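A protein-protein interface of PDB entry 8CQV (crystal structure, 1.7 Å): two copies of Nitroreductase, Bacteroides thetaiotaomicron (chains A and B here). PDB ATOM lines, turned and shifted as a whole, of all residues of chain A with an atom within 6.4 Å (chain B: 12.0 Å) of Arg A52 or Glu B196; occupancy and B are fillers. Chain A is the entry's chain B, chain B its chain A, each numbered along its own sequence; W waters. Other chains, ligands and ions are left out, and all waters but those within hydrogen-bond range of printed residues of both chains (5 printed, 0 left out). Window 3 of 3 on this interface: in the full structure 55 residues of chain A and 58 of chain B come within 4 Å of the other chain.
O of Val A54 lies within hydrogen-bond range of N of Leu A100 (2.8 Å). The side-chain carboxylate (OD2) of Asp A104 is in salt-bridge range of the guanidinium group (NH2) of Arg A52, 3.1 Å away. The backbone carbonyl oxygen (O) of Glu B195 sits at hydrogen-bond distance from the side-chain amino group (NZ) of Lys B199, at 2.8 Å. The backbone carbonyl oxygen (O) of Gln B192 is in hydrogen-bond range of the guanidinium group (NH2) of Arg B197. The backbone NH (N) of Phe A102 sits at hydrogen-bond distance from the backbone carbonyl oxygen (O) of Arg A52 (2.8 Å). O of Gln A49 is in hydrogen-bond range of NH1 of Arg A52 (2.7 Å).
Printed residues of chain B within 4 Å of Val A39: Leu B194 (3.6 Å), Arg B197 (3.4 Å) and Ile B198 (3.8 Å). Printed residues of chain B within 4 Å of Gln A49: Glu B190, Phe B191, Gln B192 and Arg B197. No residue of chain B comes within 4 Å of Ser A50. Thr A51 touches none of the printed residues of chain B. Of chain B, only Glu B196 and Arg B197 come within 4 Å of Arg A52. Of chain B, only Lys B199 (3.3 Å) and Phe B201 (3.8 Å) come within 4 Å of Val A54. Leu A100 touches none of the printed residues of chain B. No residue of chain B comes within 4 Å of Phe A101. No residue of chain B comes within 4 Å of Phe A102. No residue of chain B comes within 4 Å of Glu A103. Of chain B, only Glu B196 (3.8 Å) comes within 4 Å of Trp A171. Of the printed residues of chain A, Glu B190 touches Gln A49. Of the printed residues of chain A, Phe B191 touches Gln A49 (3.6 Å). Of chain A, only Arg A52 and Trp A171 come within 4 Å of Glu B196. Printed residues of chain A within 4 Å of Arg B197: Val A39 (3.4 Å), Gln A49 (3.2 Å), Arg A52 (3.2 Å) and Val A53 (2.9 Å). Printed residues of chain A within 4 Å of Ile B198: Val A39 (3.8 Å) and Val A53 (3.2 Å). The nearest residue of chain B that does not touch Arg A52 is Ile B198 (5.5 Å).
Water W5 bridges O of Val A39 and NH1 of Arg B197. Water W4 lies within hydrogen-bond range of NH1 of Arg B197 (2.8 Å), O of Thr A51 (2.8 Å) and O of Gln A49 (3.4 Å). Water W3 lies within hydrogen-bond range of O of Glu B190 (2.8 Å) and OE1 of Gln A49 (3.4 Å). Water W2 lies within hydrogen-bond range of NE2 of Gln A49 (2.8 Å), OE1 of Gln B192 (2.9 Å) and OE1 of Glu B190 (3.4 Å). Water W1 lies within hydrogen-bond range of NH1 of Arg B197 (2.9 Å), O of Val A39 (3.0 Å) and OE1 of Gln A49 (3.5 Å).
No position is printed for both chains. Of the 15 pairs that touch across the chains among the printed residues, none has its exchanged pair printed and touching as well.
Hydrophobic or aromatic side chains of chain A within 4 Å of the printed part of chain B: Val A39, Val A54 and Trp A171. Along chain B the printed residues that touch a printed residue of chain A span positions 190 to 201. Among the printed residues, no Asp or Glu carboxylate lies within 4 Å of a Lys or Arg side-chain nitrogen of the other chain.
The backbone carbonyl oxygen (O) of Arg B197 sits at hydrogen-bond distance from the backbone NH (N) of Val A53, 2.9 Å away. OE1 of Gln A49 lies within hydrogen-bond range of NH2 of Arg B197, at 3.2 Å. The side-chain amide oxygen of Gln A49 lies within hydrogen-bond range of the backbone NH of Gln B192 (2.7 Å). NE2 of Gln A49 lies within hydrogen-bond range of O of Glu B190. The backbone NH of Lys B199 sits at hydrogen-bond distance from the backbone carbonyl oxygen of Val A53, at 3.0 Å. O of Val A39 lies within hydrogen-bond range of NH1 of Arg B197.
Among the printed residues, pairs that only touch across the chains: Val A53 with Ile B198 (3.2 Å), Arg A52 with Arg B197 (3.2 Å), Val A54 with Lys B199 (3.3 Å), Gln A49 with Phe B191 (3.6 Å), Val A39 with Leu B194 (3.6 Å), Val A39 with Ile B198 (3.8 Å), Val A54 with Phe B201 (3.8 Å), Trp A171 with Glu B196 (3.8 Å) and Arg A52 with Glu B196 (3.9 Å).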
ATOM      1  N   VAL A  39       7.013 -18.258   9.508  1.00  0.00           N
ATOM      2  CA  VAL A  39       6.973 -16.836   9.126  1.00  0.00           C
ATOM      3  C   VAL A  39       7.874 -16.021  10.048  1.00  0.00           C
ATOM      4  O   VAL A  39       8.469 -15.050   9.589  1.00  0.00           O
ATOM      5  CB  VAL A  39       5.528 -16.294   9.027  1.00  0.00           C
ATOM      6  CG1 VAL A  39       5.515 -14.797   8.735  1.00  0.00           C
ATOM      7  CG2 VAL A  39       4.806 -17.041   7.918  1.00  0.00           C
ATOM      8  N   SER A  48      13.304  -8.361   4.740  1.00  0.00           N
ATOM      9  CA  SER A  48      12.206  -7.661   4.114  1.00  0.00           C
ATOM     10  C   SER A  48      10.850  -8.285   4.424  1.00  0.00           C
ATOM     11  O   SER A  48       9.846  -7.577   4.314  1.00  0.00           O
ATOM     12  CB  SER A  48      12.381  -7.604   2.629  1.00  0.00           C
ATOM     13  OG  SER A  48      12.592  -8.881   2.093  1.00  0.00           O
ATOM     14  N   GLN A  49      10.795  -9.566   4.834  1.00  0.00           N
ATOM     15  CA  GLN A  49       9.548 -10.141   5.313  1.00  0.00           C
ATOM     16  C   GLN A  49       8.420  -9.930   4.299  1.00  0.00           C
ATOM     17  O   GLN A  49       7.369  -9.334   4.604  1.00  0.00           O
ATOM     18  CB  GLN A  49       9.211  -9.534   6.677  1.00  0.00           C
ATOM     19  CG  GLN A  49      10.229  -9.878   7.744  1.00  0.00           C
ATOM     20  CD  GLN A  49      10.066  -9.004   8.973  1.00  0.00           C
ATOM     21  OE1 GLN A  49       9.087  -9.163   9.658  1.00  0.00           O
ATOM     22  NE2 GLN A  49      10.879  -7.923   9.107  1.00  0.00           N
ATOM     23  N   SER A  50       8.653 -10.407   3.079  1.00  0.00           N
ATOM     24  CA  SER A  50       7.692 -10.284   1.991  1.00  0.00           C
ATOM     25  C   SER A  50       6.662 -11.420   2.011  1.00  0.00           C
ATOM     26  O   SER A  50       5.690 -11.321   1.287  1.00  0.00           O
ATOM     27  CB  SER A  50       8.445 -10.269   0.669  1.00  0.00           C
ATOM     28  OG  SER A  50       9.309 -11.432   0.567  1.00  0.00           O
ATOM     29  N   THR A  51       6.875 -12.498   2.781  1.00  0.00           N
ATOM     30  CA  THR A  51       6.091 -13.715   2.678  1.00  0.00           C
ATOM     31  C   THR A  51       4.783 -13.450   3.430  1.00  0.00           C
ATOM     32  O   THR A  51       4.778 -12.907   4.559  1.00  0.00           O
ATOM     33  CB  THR A  51       6.841 -14.935   3.209  1.00  0.00           C
ATOM     34  OG1 THR A  51       8.000 -15.137   2.405  1.00  0.00           O
ATOM     35  CG2 THR A  51       6.055 -16.242   3.232  1.00  0.00           C
ATOM     36  N   ARG A  52       3.684 -13.928   2.806  1.00  0.00           N
ATOM     37  CA  ARG A  52       2.329 -13.873   3.421  1.00  0.00           C
ATOM     38  C   ARG A  52       1.738 -15.267   3.293  1.00  0.00           C
ATOM     39  O   ARG A  52       1.864 -15.906   2.230  1.00  0.00           O
ATOM     40  CB  ARG A  52       1.477 -12.834   2.706  1.00  0.00           C
ATOM     41  CG  ARG A  52       2.108 -11.466   2.572  1.00  0.00           C
ATOM     42  CD  ARG A  52       2.028 -10.710   3.856  1.00  0.00           C
ATOM     43  NE  ARG A  52       2.640  -9.386   3.782  1.00  0.00           N
ATOM     44  CZ  ARG A  52       3.926  -9.129   4.127  1.00  0.00           C
ATOM     45  NH1 ARG A  52       4.734 -10.093   4.560  1.00  0.00           N
ATOM     46  NH2 ARG A  52       4.385  -7.881   4.029  1.00  0.00           N
ATOM     47  N   VAL A  53       1.236 -15.833   4.400  1.00  0.00           N
ATOM     48  CA  VAL A  53       0.701 -17.184   4.371  1.00  0.00           C
ATOM     49  C   VAL A  53      -0.787 -17.141   4.757  1.00  0.00           C
ATOM     50  O   VAL A  53      -1.175 -16.499   5.751  1.00  0.00           O
ATOM     51  CB  VAL A  53       1.500 -18.119   5.262  1.00  0.00           C
ATOM     52  CG1 VAL A  53       0.899 -19.505   5.220  1.00  0.00           C
ATOM     53  CG2 VAL A  53       2.985 -18.127   4.869  1.00  0.00           C
ATOM     54  N   VAL A  54      -1.574 -17.860   4.003  1.00  0.00           N
ATOM     55  CA  VAL A  54      -3.011 -17.998   4.298  1.00  0.00           C
ATOM     56  C   VAL A  54      -3.275 -19.480   4.518  1.00  0.00           C
ATOM     57  O   VAL A  54      -2.988 -20.307   3.645  1.00  0.00           O
ATOM     58  CB  VAL A  54      -3.920 -17.500   3.192  1.00  0.00           C
ATOM     59  CG1 VAL A  54      -5.395 -17.821   3.462  1.00  0.00           C
ATOM     60  CG2 VAL A  54      -3.750 -16.005   2.999  1.00  0.00           C
ATOM     61  N   LEU A 100      -1.657 -21.608   1.526  1.00  0.00           N
ATOM     62  CA  LEU A 100      -1.354 -20.761   0.409  1.00  0.00           C
ATOM     63  C   LEU A 100      -0.175 -19.860   0.753  1.00  0.00           C
ATOM     64  O   LEU A 100      -0.146 -19.166   1.795  1.00  0.00           O
ATOM     65  CB  LEU A 100      -2.560 -19.902   0.046  1.00  0.00           C
ATOM     66  CG  LEU A 100      -3.855 -20.636  -0.256  1.00  0.00           C
ATOM     67  CD1 LEU A 100      -4.949 -19.594  -0.520  1.00  0.00           C
ATOM     68  CD2 LEU A 100      -3.713 -21.553  -1.448  1.00  0.00           C
ATOM     69  N   PHE A 101       0.780 -19.808  -0.205  1.00  0.00           N
ATOM     70  CA  PHE A 101       1.961 -18.979  -0.043  1.00  0.00           C
ATOM     71  C   PHE A 101       1.894 -17.813  -0.993  1.00  0.00           C
ATOM     72  O   PHE A 101       1.820 -18.025  -2.235  1.00  0.00           O
ATOM     73  CB  PHE A 101       3.218 -19.847  -0.306  1.00  0.00           C
ATOM     74  CG  PHE A 101       3.385 -21.005   0.648  1.00  0.00           C
ATOM     75  CD1 PHE A 101       2.772 -22.208   0.420  1.00  0.00           C
ATOM     76  CD2 PHE A 101       4.149 -20.879   1.821  1.00  0.00           C
ATOM     77  CE1 PHE A 101       2.887 -23.255   1.315  1.00  0.00           C
ATOM     78  CE2 PHE A 101       4.299 -21.929   2.695  1.00  0.00           C
ATOM     79  CZ  PHE A 101       3.619 -23.124   2.474  1.00  0.00           C
ATOM     80  N   PHE A 102       1.947 -16.605  -0.441  1.00  0.00           N
ATOM     81  CA  PHE A 102       2.005 -15.415  -1.276  1.00  0.00           C
ATOM     82  C   PHE A 102       3.269 -14.593  -0.995  1.00  0.00           C
ATOM     83  O   PHE A 102       3.856 -14.680   0.070  1.00  0.00           O
ATOM     84  CB  PHE A 102       0.819 -14.505  -0.940  1.00  0.00           C
ATOM     85  CG  PHE A 102      -0.580 -15.044  -1.132  1.00  0.00           C
ATOM     86  CD1 PHE A 102      -1.160 -15.897  -0.199  1.00  0.00           C
ATOM     87  CD2 PHE A 102      -1.247 -14.767  -2.319  1.00  0.00           C
ATOM     88  CE1 PHE A 102      -2.471 -16.335  -0.388  1.00  0.00           C
ATOM     89  CE2 PHE A 102      -2.564 -15.213  -2.485  1.00  0.00           C
ATOM     90  CZ  PHE A 102      -3.146 -16.021  -1.537  1.00  0.00           C
ATOM     91  N   GLU A 103       3.603 -13.723  -1.939  1.00  0.00           N
ATOM     92  CA  GLU A 103       4.685 -12.744  -1.824  1.00  0.00           C
ATOM     93  C   GLU A 103       4.075 -11.353  -2.027  1.00  0.00           C
ATOM     94  O   GLU A 103       3.361 -11.089  -2.998  1.00  0.00           O
ATOM     95  CB  GLU A 103       5.843 -13.081  -2.749  1.00  0.00           C
ATOM     96  CG  GLU A 103       6.647 -14.316  -2.302  1.00  0.00           C
ATOM     97  CD  GLU A 103       7.408 -14.115  -1.007  1.00  0.00           C
ATOM     98  OE1 GLU A 103       7.327 -14.950  -0.139  1.00  0.00           O
ATOM     99  OE2 GLU A 103       8.101 -13.051  -0.871  1.00  0.00           O
ATOM    100  N   ASP A 104       4.366 -10.461  -1.080  1.00  0.00           N
ATOM    101  CA  ASP A 104       3.820  -9.102  -1.050  1.00  0.00           C
ATOM    102  C   ASP A 104       4.610  -8.246  -2.024  1.00  0.00           C
ATOM    103  O   ASP A 104       5.774  -7.908  -1.765  1.00  0.00           O
ATOM    104  CB  ASP A 104       3.912  -8.524   0.354  1.00  0.00           C
ATOM    105  CG  ASP A 104       3.227  -7.160   0.494  1.00  0.00           C
ATOM    106  OD1 ASP A 104       3.224  -6.380  -0.472  1.00  0.00           O
ATOM    107  OD2 ASP A 104       2.844  -6.886   1.545  1.00  0.00           O
ATOM    108  N   VAL A 107       6.162  -4.890  -0.989  1.00  0.00           N
ATOM    109  CA  VAL A 107       7.491  -5.010  -0.393  1.00  0.00           C
ATOM    110  C   VAL A 107       8.547  -5.130  -1.492  1.00  0.00           C
ATOM    111  O   VAL A 107       9.568  -4.429  -1.442  1.00  0.00           O
ATOM    112  CB  VAL A 107       7.598  -6.158   0.600  1.00  0.00           C
ATOM    113  CG1 VAL A 107       9.025  -6.294   1.078  1.00  0.00           C
ATOM    114  CG2 VAL A 107       6.633  -5.972   1.779  1.00  0.00           C
ATOM    115  N   TRP A 171      -0.748  -9.145  -3.055  1.00  0.00           N
ATOM    116  CA  TRP A 171      -0.248 -10.465  -2.687  1.00  0.00           C
ATOM    117  C   TRP A 171      -0.256 -11.379  -3.907  1.00  0.00           C
ATOM    118  O   TRP A 171      -1.322 -11.701  -4.489  1.00  0.00           O
ATOM    119  CB  TRP A 171      -1.031 -11.082  -1.557  1.00  0.00           C
ATOM    120  CG  TRP A 171      -0.864 -10.453  -0.224  1.00  0.00           C
ATOM    121  CD1 TRP A 171      -0.314  -9.236   0.079  1.00  0.00           C
ATOM    122  CD2 TRP A 171      -1.364 -10.991   1.006  1.00  0.00           C
ATOM    123  NE1 TRP A 171      -0.431  -9.016   1.427  1.00  0.00           N
ATOM    124  CE2 TRP A 171      -1.023 -10.082   2.031  1.00  0.00           C
ATOM    125  CE3 TRP A 171      -2.056 -12.163   1.348  1.00  0.00           C
ATOM    126  CZ2 TRP A 171      -1.391 -10.277   3.366  1.00  0.00           C
ATOM    127  CZ3 TRP A 171      -2.352 -12.403   2.675  1.00  0.00           C
ATOM    128  CH2 TRP A 171      -2.033 -11.455   3.664  1.00  0.00           C
ATOM    129  N   GLN B 128      13.718 -21.954  -6.822  1.00  0.00           N
ATOM    130  CA  GLN B 128      13.055 -22.394  -5.598  1.00  0.00           C
ATOM    131  C   GLN B 128      13.731 -23.609  -4.943  1.00  0.00           C
ATOM    132  O   GLN B 128      14.006 -23.592  -3.739  1.00  0.00           O
ATOM    133  CB  GLN B 128      11.566 -22.629  -5.872  1.00  0.00           C
ATOM    134  CG  GLN B 128      10.839 -21.285  -6.115  1.00  0.00           C
ATOM    135  CD  GLN B 128       9.377 -21.604  -6.313  1.00  0.00           C
ATOM    136  OE1 GLN B 128       8.729 -21.974  -5.357  1.00  0.00           O
ATOM    137  NE2 GLN B 128       8.819 -21.421  -7.514  1.00  0.00           N
ATOM    138  N   GLU B 190      14.248  -7.271  13.610  1.00  0.00           N
ATOM    139  CA  GLU B 190      12.891  -6.733  13.675  1.00  0.00           C
ATOM    140  C   GLU B 190      11.909  -7.760  13.123  1.00  0.00           C
ATOM    141  O   GLU B 190      12.221  -8.469  12.154  1.00  0.00           O
ATOM    142  CB  GLU B 190      12.730  -5.480  12.815  1.00  0.00           C
ATOM    143  CG  GLU B 190      13.621  -4.329  13.183  1.00  0.00           C
ATOM    144  CD  GLU B 190      13.366  -3.008  12.449  1.00  0.00           C
ATOM    145  OE1 GLU B 190      12.332  -2.847  11.686  1.00  0.00           O
ATOM    146  OE2 GLU B 190      14.180  -2.107  12.704  1.00  0.00           O
ATOM    147  N   PHE B 191      10.702  -7.787  13.691  1.00  0.00           N
ATOM    148  CA  PHE B 191       9.646  -8.654  13.189  1.00  0.00           C
ATOM    149  C   PHE B 191       8.400  -7.809  12.940  1.00  0.00           C
ATOM    150  O   PHE B 191       7.893  -7.202  13.894  1.00  0.00           O
ATOM    151  CB  PHE B 191       9.327  -9.740  14.217  1.00  0.00           C
ATOM    152  CG  PHE B 191      10.447 -10.685  14.531  1.00  0.00           C
ATOM    153  CD1 PHE B 191      11.419 -10.348  15.445  1.00  0.00           C
ATOM    154  CD2 PHE B 191      10.572 -11.902  13.866  1.00  0.00           C
ATOM    155  CE1 PHE B 191      12.453 -11.230  15.745  1.00  0.00           C
ATOM    156  CE2 PHE B 191      11.610 -12.784  14.157  1.00  0.00           C
ATOM    157  CZ  PHE B 191      12.572 -12.426  15.072  1.00  0.00           C
ATOM    158  N   GLN B 192       7.853  -7.839  11.712  1.00  0.00           N
ATOM    159  CA  GLN B 192       6.590  -7.185  11.423  1.00  0.00           C
ATOM    160  C   GLN B 192       5.492  -7.988  12.115  1.00  0.00           C
ATOM    161  O   GLN B 192       5.661  -9.184  12.312  1.00  0.00           O
ATOM    162  CB  GLN B 192       6.299  -7.206   9.922  1.00  0.00           C
ATOM    163  CG  GLN B 192       7.180  -6.305   9.090  1.00  0.00           C
ATOM    164  CD  GLN B 192       7.006  -4.861   9.460  1.00  0.00           C
ATOM    165  OE1 GLN B 192       7.911  -4.261  10.026  1.00  0.00           O
ATOM    166  NE2 GLN B 192       5.808  -4.335   9.249  1.00  0.00           N
ATOM    167  N   PRO B 193       4.368  -7.367  12.531  1.00  0.00           N
ATOM    168  CA  PRO B 193       3.298  -8.105  13.204  1.00  0.00           C
ATOM    169  C   PRO B 193       2.858  -9.346  12.418  1.00  0.00           C
ATOM    170  O   PRO B 193       2.687  -9.257  11.196  1.00  0.00           O
ATOM    171  CB  PRO B 193       2.186  -7.060  13.268  1.00  0.00           C
ATOM    172  CG  PRO B 193       3.015  -5.801  13.493  1.00  0.00           C
ATOM    173  CD  PRO B 193       4.098  -5.922  12.429  1.00  0.00           C
ATOM    174  N   LEU B 194       2.828 -10.517  13.081  1.00  0.00           N
ATOM    175  CA  LEU B 194       2.457 -11.759  12.410  1.00  0.00           C
ATOM    176  C   LEU B 194       1.004 -11.709  11.867  1.00  0.00           C
ATOM    177  O   LEU B 194       0.697 -12.309  10.813  1.00  0.00           O
ATOM    178  CB  LEU B 194       2.705 -12.936  13.356  1.00  0.00           C
ATOM    179  CG  LEU B 194       4.155 -13.436  13.472  1.00  0.00           C
ATOM    180  CD1 LEU B 194       4.661 -14.001  12.182  1.00  0.00           C
ATOM    181  CD2 LEU B 194       5.175 -12.394  13.940  1.00  0.00           C
ATOM    182  N   GLU B 195       0.098 -11.000  12.543  1.00  0.00           N
ATOM    183  CA  GLU B 195      -1.283 -10.935  12.052  1.00  0.00           C
ATOM    184  C   GLU B 195      -1.434 -10.082  10.776  1.00  0.00           C
ATOM    185  O   GLU B 195      -2.455 -10.220  10.103  1.00  0.00           O
ATOM    186  CB  GLU B 195      -2.268 -10.554  13.152  1.00  0.00           C
ATOM    187  CG  GLU B 195      -2.209  -9.132  13.577  1.00  0.00           C
ATOM    188  CD  GLU B 195      -1.405  -8.961  14.849  1.00  0.00           C
ATOM    189  OE1 GLU B 195      -1.985  -8.485  15.837  1.00  0.00           O
ATOM    190  OE2 GLU B 195      -0.241  -9.376  14.850  1.00  0.00           O
ATOM    191  N   GLU B 196      -0.446  -9.250  10.388  1.00  0.00           N
ATOM    192  CA  GLU B 196      -0.445  -8.624   9.075  1.00  0.00           C
ATOM    193  C   GLU B 196       0.035  -9.614   8.006  1.00  0.00           C
ATOM    194  O   GLU B 196      -0.065  -9.288   6.834  1.00  0.00           O
ATOM    195  CB  GLU B 196       0.419  -7.364   9.061  1.00  0.00           C
ATOM    196  CG  GLU B 196      -0.151  -6.267   9.912  1.00  0.00           C
ATOM    197  CD  GLU B 196       0.780  -5.077  10.078  1.00  0.00           C
ATOM    198  OE1 GLU B 196       1.817  -5.016   9.376  1.00  0.00           O
ATOM    199  OE2 GLU B 196       0.497  -4.234  10.967  1.00  0.00           O
ATOM    200  N   ARG B 197       0.675 -10.720   8.389  1.00  0.00           N
ATOM    201  CA  ARG B 197       1.379 -11.596   7.442  1.00  0.00           C
ATOM    202  C   ARG B 197       0.777 -12.997   7.331  1.00  0.00           C
ATOM    203  O   ARG B 197       1.178 -13.721   6.419  1.00  0.00           O
ATOM    204  CB  ARG B 197       2.849 -11.712   7.858  1.00  0.00           C
ATOM    205  CG  ARG B 197       3.512 -10.343   7.877  1.00  0.00           C
ATOM    206  CD  ARG B 197       4.985 -10.447   7.995  1.00  0.00           C
ATOM    207  NE  ARG B 197       5.394 -10.824   9.348  1.00  0.00           N
ATOM    208  CZ  ARG B 197       6.620 -11.292   9.659  1.00  0.00           C
ATOM    209  NH1 ARG B 197       7.377 -11.910   8.763  1.00  0.00           N
ATOM    210  NH2 ARG B 197       7.005 -11.202  10.932  1.00  0.00           N
ATOM    211  N   ILE B 198      -0.114 -13.392   8.270  1.00  0.00           N
ATOM    212  CA  ILE B 198      -0.737 -14.709   8.320  1.00  0.00           C
ATOM    213  C   ILE B 198      -2.222 -14.479   8.493  1.00  0.00           C
ATOM    214  O   ILE B 198      -2.617 -13.680   9.366  1.00  0.00           O
ATOM    215  CB  ILE B 198      -0.168 -15.564   9.456  1.00  0.00           C
ATOM    216  CG1 ILE B 198       1.346 -15.758   9.316  1.00  0.00           C
ATOM    217  CG2 ILE B 198      -0.903 -16.881   9.553  1.00  0.00           C
ATOM    218  CD1 ILE B 198       2.049 -16.207  10.585  1.00  0.00           C
ATOM    219  N   LYS B 199      -3.043 -15.138   7.652  1.00  0.00           N
ATOM    220  CA  LYS B 199      -4.501 -15.158   7.823  1.00  0.00           C
ATOM    221  C   LYS B 199      -4.949 -16.607   7.897  1.00  0.00           C
ATOM    222  O   LYS B 199      -4.386 -17.482   7.218  1.00  0.00           O
ATOM    223  CB  LYS B 199      -5.195 -14.470   6.653  1.00  0.00           C
ATOM    224  CG  LYS B 199      -4.783 -13.024   6.455  1.00  0.00           C
ATOM    225  CD  LYS B 199      -5.193 -12.132   7.592  1.00  0.00           C
ATOM    226  CE  LYS B 199      -4.295 -10.925   7.671  1.00  0.00           C
ATOM    227  NZ  LYS B 199      -4.856  -9.948   8.625  1.00  0.00           N
ATOM    228  N   VAL B 200      -5.947 -16.862   8.739  1.00  0.00           N
ATOM    229  CA  VAL B 200      -6.511 -18.207   8.887  1.00  0.00           C
ATOM    230  C   VAL B 200      -8.010 -18.077   8.677  1.00  0.00           C
ATOM    231  O   VAL B 200      -8.626 -17.210   9.281  1.00  0.00           O
ATOM    232  CB  VAL B 200      -6.186 -18.881  10.232  1.00  0.00           C
ATOM    233  CG1 VAL B 200      -6.716 -20.325  10.277  1.00  0.00           C
ATOM    234  CG2 VAL B 200      -4.716 -18.852  10.527  1.00  0.00           C
ATOM    235  N   PHE B 201      -8.575 -18.873   7.755  1.00  0.00           N
ATOM    236  CA  PHE B 201     -10.004 -18.864   7.450  1.00  0.00           C
ATOM    237  C   PHE B 201     -10.504 -20.289   7.537  1.00  0.00           C
ATOM    238  O   PHE B 201      -9.848 -21.160   7.018  1.00  0.00           O
ATOM    239  CB  PHE B 201     -10.206 -18.370   6.020  1.00  0.00           C
ATOM    240  CG  PHE B 201      -9.768 -16.936   5.834  1.00  0.00           C
ATOM    241  CD1 PHE B 201     -10.564 -15.903   6.310  1.00  0.00           C
ATOM    242  CD2 PHE B 201      -8.599 -16.626   5.180  1.00  0.00           C
ATOM    243  CE1 PHE B 201     -10.144 -14.593   6.159  1.00  0.00           C
ATOM    244  CE2 PHE B 201      -8.216 -15.308   4.995  1.00  0.00           C
ATOM    245  CZ  PHE B 201      -9.000 -14.297   5.481  1.00  0.00           C
HETATM  246  O   HOH W   1       9.689 -12.480  10.493  1.00  0.00           O
HETATM  247  O   HOH W   2      10.611  -5.341  10.233  1.00  0.00           O
HETATM  248  O   HOH W   3      11.838 -10.814  10.727  1.00  0.00           O
HETATM  249  O   HOH W   4       7.125 -12.365   6.043  1.00  0.00           O
HETATM  250  O   HOH W   5       8.679 -14.528   7.108  1.00  0.00           O
